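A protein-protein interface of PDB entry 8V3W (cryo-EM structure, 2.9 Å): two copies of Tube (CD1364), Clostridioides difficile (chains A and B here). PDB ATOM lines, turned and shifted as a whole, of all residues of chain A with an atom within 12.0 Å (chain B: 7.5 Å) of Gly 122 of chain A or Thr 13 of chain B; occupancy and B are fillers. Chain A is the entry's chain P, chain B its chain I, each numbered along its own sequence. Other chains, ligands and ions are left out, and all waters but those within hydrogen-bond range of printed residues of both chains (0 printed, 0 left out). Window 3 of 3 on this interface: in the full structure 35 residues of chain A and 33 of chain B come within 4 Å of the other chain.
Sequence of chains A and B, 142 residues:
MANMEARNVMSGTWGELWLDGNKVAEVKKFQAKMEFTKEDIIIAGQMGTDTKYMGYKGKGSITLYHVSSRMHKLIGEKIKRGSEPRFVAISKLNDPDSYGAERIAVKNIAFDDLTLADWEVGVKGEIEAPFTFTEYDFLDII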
ATOM      1  N   HIS A  66      19.078  21.928  20.688  1.00  0.00           N
ATOM      2  CA  HIS A  66      19.747  21.415  19.496  1.00  0.00           C
ATOM      3  C   HIS A  66      20.546  20.173  19.871  1.00  0.00           C
ATOM      4  O   HIS A  66      21.674  20.268  20.354  1.00  0.00           O
ATOM      5  CB  HIS A  66      20.634  22.482  18.871  1.00  0.00           C
ATOM      6  CG  HIS A  66      21.199  22.088  17.545  1.00  0.00           C
ATOM      7  ND1 HIS A  66      20.476  21.386  16.607  1.00  0.00           N
ATOM      8  CD2 HIS A  66      22.419  22.295  17.000  1.00  0.00           C
ATOM      9  CE1 HIS A  66      21.225  21.180  15.540  1.00  0.00           C
ATOM     10  NE2 HIS A  66      22.410  21.719  15.753  1.00  0.00           N
ATOM     11  N   ASP A 118      23.273  27.716  13.497  1.00  0.00           N
ATOM     12  CA  ASP A 118      23.261  28.920  14.326  1.00  0.00           C
ATOM     13  C   ASP A 118      24.009  28.588  15.618  1.00  0.00           C
ATOM     14  O   ASP A 118      23.415  28.098  16.580  1.00  0.00           O
ATOM     15  CB  ASP A 118      21.836  29.386  14.591  1.00  0.00           C
ATOM     16  CG  ASP A 118      21.765  30.528  15.582  1.00  0.00           C
ATOM     17  OD1 ASP A 118      22.606  31.446  15.504  1.00  0.00           O
ATOM     18  OD2 ASP A 118      20.860  30.511  16.440  1.00  0.00           O
ATOM     19  N   TRP A 119      25.310  28.864  15.629  1.00  0.00           N
ATOM     20  CA  TRP A 119      26.139  28.565  16.785  1.00  0.00           C
ATOM     21  C   TRP A 119      27.073  29.732  17.068  1.00  0.00           C
ATOM     22  O   TRP A 119      27.350  30.560  16.201  1.00  0.00           O
ATOM     23  CB  TRP A 119      26.940  27.264  16.604  1.00  0.00           C
ATOM     24  CG  TRP A 119      27.738  27.142  15.339  1.00  0.00           C
ATOM     25  CD1 TRP A 119      27.328  26.585  14.167  1.00  0.00           C
ATOM     26  CD2 TRP A 119      29.097  27.548  15.134  1.00  0.00           C
ATOM     27  NE1 TRP A 119      28.336  26.633  13.241  1.00  0.00           N
ATOM     28  CE2 TRP A 119      29.433  27.220  13.809  1.00  0.00           C
ATOM     29  CE3 TRP A 119      30.055  28.171  15.937  1.00  0.00           C
ATOM     30  CZ2 TRP A 119      30.684  27.492  13.268  1.00  0.00           C
ATOM     31  CZ3 TRP A 119      31.297  28.437  15.399  1.00  0.00           C
ATOM     32  CH2 TRP A 119      31.602  28.098  14.078  1.00  0.00           C
ATOM     33  N   GLU A 120      27.541  29.787  18.312  1.00  0.00           N
ATOM     34  CA  GLU A 120      28.434  30.829  18.793  1.00  0.00           C
ATOM     35  C   GLU A 120      29.301  30.237  19.890  1.00  0.00           C
ATOM     36  O   GLU A 120      28.850  29.374  20.643  1.00  0.00           O
ATOM     37  CB  GLU A 120      27.655  32.031  19.325  1.00  0.00           C
ATOM     38  CG  GLU A 120      28.522  33.206  19.697  1.00  0.00           C
ATOM     39  CD  GLU A 120      27.822  34.184  20.602  1.00  0.00           C
ATOM     40  OE1 GLU A 120      26.608  34.405  20.422  1.00  0.00           O
ATOM     41  OE2 GLU A 120      28.489  34.743  21.494  1.00  0.00           O
ATOM     42  N   VAL A 121      30.546  30.704  19.984  1.00  0.00           N
ATOM     43  CA  VAL A 121      31.471  30.129  20.952  1.00  0.00           C
ATOM     44  C   VAL A 121      31.000  30.452  22.363  1.00  0.00           C
ATOM     45  O   VAL A 121      30.695  31.605  22.687  1.00  0.00           O
ATOM     46  CB  VAL A 121      32.908  30.620  20.705  1.00  0.00           C
ATOM     47  CG1 VAL A 121      33.460  30.026  19.421  1.00  0.00           C
ATOM     48  CG2 VAL A 121      32.979  32.136  20.669  1.00  0.00           C
ATOM     49  N   GLY A 122      30.920  29.425  23.206  1.00  0.00           N
ATOM     50  CA  GLY A 122      30.509  29.588  24.583  1.00  0.00           C
ATOM     51  C   GLY A 122      29.020  29.660  24.827  1.00  0.00           C
ATOM     52  O   GLY A 122      28.612  30.085  25.911  1.00  0.00           O
ATOM     53  N   VAL A 123      28.192  29.270  23.860  1.00  0.00           N
ATOM     54  CA  VAL A 123      26.740  29.345  23.972  1.00  0.00           C
ATOM     55  C   VAL A 123      26.144  28.008  23.547  1.00  0.00           C
ATOM     56  O   VAL A 123      26.584  27.411  22.561  1.00  0.00           O
ATOM     57  CB  VAL A 123      26.166  30.493  23.112  1.00  0.00           C
ATOM     58  CG1 VAL A 123      24.667  30.593  23.281  1.00  0.00           C
ATOM     59  CG2 VAL A 123      26.826  31.810  23.465  1.00  0.00           C
ATOM     60  N   LYS A 124      25.146  27.537  24.291  1.00  0.00           N
ATOM     61  CA  LYS A 124      24.474  26.287  23.962  1.00  0.00           C
ATOM     62  C   LYS A 124      23.374  26.521  22.934  1.00  0.00           C
ATOM     63  O   LYS A 124      22.740  27.578  22.913  1.00  0.00           O
ATOM     64  CB  LYS A 124      23.896  25.644  25.222  1.00  0.00           C
ATOM     65  CG  LYS A 124      22.888  26.503  25.960  1.00  0.00           C
ATOM     66  CD  LYS A 124      21.705  25.680  26.417  1.00  0.00           C
ATOM     67  CE  LYS A 124      20.768  26.496  27.282  1.00  0.00           C
ATOM     68  NZ  LYS A 124      19.757  27.220  26.473  1.00  0.00           N
ATOM     69  N   GLY A 125      23.155  25.530  22.075  1.00  0.00           N
ATOM     70  CA  GLY A 125      22.332  25.718  20.896  1.00  0.00           C
ATOM     71  C   GLY A 125      20.847  25.475  21.107  1.00  0.00           C
ATOM     72  O   GLY A 125      20.445  24.589  21.850  1.00  0.00           O
ATOM     73  N   GLU A 126      20.037  26.272  20.410  1.00  0.00           N
ATOM     74  CA  GLU A 126      18.587  26.145  20.420  1.00  0.00           C
ATOM     75  C   GLU A 126      18.038  26.442  19.031  1.00  0.00           C
ATOM     76  O   GLU A 126      18.666  27.130  18.226  1.00  0.00           O
ATOM     77  CB  GLU A 126      17.937  27.084  21.439  1.00  0.00           C
ATOM     78  CG  GLU A 126      18.219  26.730  22.879  1.00  0.00           C
ATOM     79  CD  GLU A 126      17.739  27.792  23.837  1.00  0.00           C
ATOM     80  OE1 GLU A 126      17.151  28.792  23.375  1.00  0.00           O
ATOM     81  OE2 GLU A 126      17.941  27.624  25.058  1.00  0.00           O
ATOM     82  N   MET B  10      24.492  20.537  21.967  1.00  0.00           N
ATOM     83  CA  MET B  10      25.727  20.915  21.299  1.00  0.00           C
ATOM     84  C   MET B  10      26.216  22.269  21.792  1.00  0.00           C
ATOM     85  O   MET B  10      25.458  23.241  21.827  1.00  0.00           O
ATOM     86  CB  MET B  10      25.517  20.953  19.790  1.00  0.00           C
ATOM     87  CG  MET B  10      24.922  19.690  19.216  1.00  0.00           C
ATOM     88  SD  MET B  10      25.343  19.463  17.488  1.00  0.00           S
ATOM     89  CE  MET B  10      23.983  18.437  16.958  1.00  0.00           C
ATOM     90  N   SER B  11      27.489  22.334  22.158  1.00  0.00           N
ATOM     91  CA  SER B  11      28.119  23.580  22.557  1.00  0.00           C
ATOM     92  C   SER B  11      28.771  24.235  21.349  1.00  0.00           C
ATOM     93  O   SER B  11      29.412  23.567  20.536  1.00  0.00           O
ATOM     94  CB  SER B  11      29.158  23.332  23.648  1.00  0.00           C
ATOM     95  OG  SER B  11      30.108  24.377  23.695  1.00  0.00           O
ATOM     96  N   GLY B  12      28.607  25.551  21.239  1.00  0.00           N
ATOM     97  CA  GLY B  12      29.102  26.261  20.077  1.00  0.00           C
ATOM     98  C   GLY B  12      30.600  26.434  20.037  1.00  0.00           C
ATOM     99  O   GLY B  12      31.132  26.796  18.984  1.00  0.00           O
ATOM    100  N   THR B  13      31.292  26.186  21.147  1.00  0.00           N
ATOM    101  CA  THR B  13      32.748  26.241  21.143  1.00  0.00           C
ATOM    102  C   THR B  13      33.348  25.203  20.207  1.00  0.00           C
ATOM    103  O   THR B  13      34.475  25.380  19.738  1.00  0.00           O
ATOM    104  CB  THR B  13      33.279  26.042  22.564  1.00  0.00           C
ATOM    105  OG1 THR B  13      32.576  26.906  23.458  1.00  0.00           O
ATOM    106  CG2 THR B  13      34.751  26.369  22.645  1.00  0.00           C
ATOM    107  N   TRP B  14      32.610  24.139  19.908  1.00  0.00           N
ATOM    108  CA  TRP B  14      33.091  23.058  19.066  1.00  0.00           C
ATOM    109  C   TRP B  14      32.771  23.258  17.589  1.00  0.00           C
ATOM    110  O   TRP B  14      32.733  22.280  16.839  1.00  0.00           O
ATOM    111  CB  TRP B  14      32.523  21.730  19.563  1.00  0.00           C
ATOM    112  CG  TRP B  14      33.110  21.318  20.865  1.00  0.00           C
ATOM    113  CD1 TRP B  14      32.479  21.264  22.066  1.00  0.00           C
ATOM    114  CD2 TRP B  14      34.460  20.909  21.101  1.00  0.00           C
ATOM    115  NE1 TRP B  14      33.349  20.846  23.039  1.00  0.00           N
ATOM    116  CE2 TRP B  14      34.574  20.621  22.472  1.00  0.00           C
ATOM    117  CE3 TRP B  14      35.583  20.757  20.286  1.00  0.00           C
ATOM    118  CZ2 TRP B  14      35.763  20.189  23.045  1.00  0.00           C
ATOM    119  CZ3 TRP B  14      36.763  20.332  20.857  1.00  0.00           C
ATOM    120  CH2 TRP B  14      36.844  20.049  22.221  1.00  0.00           C
ATOM    121  N   GLY B  15      32.552  24.496  17.152  1.00  0.00           N
ATOM    122  CA  GLY B  15      32.299  24.771  15.752  1.00  0.00           C
ATOM    123  C   GLY B  15      33.566  25.078  14.972  1.00  0.00           C
ATOM    124  O   GLY B  15      34.571  25.502  15.529  1.00  0.00           O
ATOM    125  N   GLU B  16      33.507  24.841  13.663  1.00  0.00           N
ATOM    126  CA  GLU B  16      34.598  25.167  12.756  1.00  0.00           C
ATOM    127  C   GLU B  16      34.025  25.679  11.444  1.00  0.00           C
ATOM    128  O   GLU B  16      32.908  25.335  11.058  1.00  0.00           O
ATOM    129  CB  GLU B  16      35.504  23.958  12.501  1.00  0.00           C
ATOM    130  CG  GLU B  16      36.719  23.907  13.400  1.00  0.00           C
ATOM    131  CD  GLU B  16      37.256  22.506  13.579  1.00  0.00           C
ATOM    132  OE1 GLU B  16      36.715  21.769  14.425  1.00  0.00           O
ATOM    133  OE2 GLU B  16      38.222  22.142  12.880  1.00  0.00           O
ATOM    134  N   LYS B  28      33.749  33.582  15.354  1.00  0.00           N
ATOM    135  CA  LYS B  28      33.014  33.777  16.596  1.00  0.00           C
ATOM    136  C   LYS B  28      31.620  33.169  16.556  1.00  0.00           C
ATOM    137  O   LYS B  28      31.204  32.523  17.518  1.00  0.00           O
ATOM    138  CB  LYS B  28      32.924  35.274  16.917  1.00  0.00           C
ATOM    139  CG  LYS B  28      32.646  35.583  18.367  1.00  0.00           C
ATOM    140  CD  LYS B  28      32.984  37.021  18.688  1.00  0.00           C
ATOM    141  CE  LYS B  28      32.637  37.355  20.124  1.00  0.00           C
ATOM    142  NZ  LYS B  28      31.176  37.520  20.311  1.00  0.00           N
ATOM    143  N   LEU B  93      30.093  21.186  13.194  1.00  0.00           N
ATOM    144  CA  LEU B  93      29.769  21.227  14.619  1.00  0.00           C
ATOM    145  C   LEU B  93      29.933  19.810  15.159  1.00  0.00           C
ATOM    146  O   LEU B  93      29.105  18.940  14.886  1.00  0.00           O
ATOM    147  CB  LEU B  93      28.356  21.753  14.842  1.00  0.00           C
ATOM    148  CG  LEU B  93      27.975  22.303  16.212  1.00  0.00           C
ATOM    149  CD1 LEU B  93      29.069  23.167  16.786  1.00  0.00           C
ATOM    150  CD2 LEU B  93      26.684  23.080  16.107  1.00  0.00           C
ATOM    151  N   ASN B  94      30.999  19.578  15.923  1.00  0.00           N
ATOM    152  CA  ASN B  94      31.368  18.241  16.388  1.00  0.00           C
ATOM    153  C   ASN B  94      31.636  18.287  17.889  1.00  0.00           C
ATOM    154  O   ASN B  94      32.783  18.422  18.319  1.00  0.00           O
ATOM    155  CB  ASN B  94      32.580  17.732  15.624  1.00  0.00           C
ATOM    156  CG  ASN B  94      32.829  16.262  15.843  1.00  0.00           C
ATOM    157  OD1 ASN B  94      31.902  15.460  15.839  1.00  0.00           O
ATOM    158  ND2 ASN B  94      34.086  15.900  16.043  1.00  0.00           N
ATOM    159  N   ASP B  95      30.582  18.163  18.677  1.00  0.00           N
ATOM    160  CA  ASP B  95      30.713  18.104  20.127  1.00  0.00           C
ATOM    161  C   ASP B  95      31.044  16.678  20.554  1.00  0.00           C
ATOM    162  O   ASP B  95      30.345  15.745  20.155  1.00  0.00           O
ATOM    163  CB  ASP B  95      29.424  18.564  20.794  1.00  0.00           C
ATOM    164  CG  ASP B  95      29.635  19.041  22.211  1.00  0.00           C
ATOM    165  OD1 ASP B  95      29.970  18.216  23.081  1.00  0.00           O
ATOM    166  OD2 ASP B  95      29.448  20.245  22.463  1.00  0.00           O
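Of the 10 printed residues of chain A, 8 touch a printed residue of chain B.
Hydrophobic or aromatic side chains of chain A that line the printed part of chain B: His 66, Trp 119 and Val 121.
Hydrophobic or aromatic side chains of chain B that line the printed part of chain A: Met 10.
Among the printed residues, no Asp or Glu carboxylate lies within 4 Å of a Lys or Arg side-chain nitrogen of the other chain.
No position is printed for both chains.
Among the printed residues, pairs that only touch across the chains: Trp 119 of chain A with Gly 12 of chain B, Trp 119 of chain A with Gly 15 of chain B, Trp 119 of chain A with Glu 16 of chain B, Glu 120 of chain A with Gly 12 of chain B, Glu 120 of chain A with Lys 28 of chain B, Val 121 of chain A with Gly 12 of chain B, Val 121 of chain A with Thr 13 of chain B and Lys 124 of chain A with Met 10 of chain B.
Asp 118 of chain A touches none of the printed residues of chain B.
Printed residues of chain B within 4 Å of Glu 120 of chain A: Gly 12 (3.2 Å) and Lys 28 (3.5 Å).
Of the printed residues of chain B, Val 121 of chain A touches Gly 12, Thr 13 and Lys 28.
Of chain B, only Thr 13 comes within 4 Å of Gly 122 of chain A.
Of the printed residues of chain B, Lys 124 of chain A touches Met 10 (3.8 Å).
Of chain A, only Trp 119, Glu 120, Val 121 and Val 123 come within 4 Å of Gly 12 of chain B.
Thr 13 of chain B touches two residues of chain A.
No residue of chain A comes within 4 Å of Trp 14 of chain B.
Of chain A, only Trp 119 comes within 4 Å of Gly 15 of chain B.
Of the printed residues of chain A, Lys 28 of chain B touches Glu 120 and Val 121.
The nearest printed residue of chain A that does not touch Glu 16 of chain B is Val 121 of chain A (7.7 Å).
The backbone carbonyl oxygen (O) of His 66 of chain A lies within hydrogen-bond range of the backbone NH (N) of Met 10 of chain B, at 3.3 Å.
The backbone carbonyl oxygen (O) of Met 10 of chain B is in hydrogen-bond range of the backbone NH (N) of Gly 125 of chain A (3.3 Å).
The backbone NH of Gly 12 of chain B is in hydrogen-bond range of the backbone carbonyl oxygen of Val 123 of chain A (3.0 Å).
OG1 of Thr 13 of chain B is in hydrogen-bond range of N of Gly 122 of chain A, at 3.0 Å.
The backbone NH (N) of Val 121 of chain A sits at hydrogen-bond distance from the backbone carbonyl oxygen (O) of Lys 28 of chain B (3.1 Å).
The side-chain hydroxyl (OG) of Ser 11 of chain B lies close to the backbone NH (N) of Thr 13 of chain B (3.3 Å).
N of His 66 of chain A lies within hydrogen-bond range of O of Gly 125 of chain A, 3.2 Å away.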
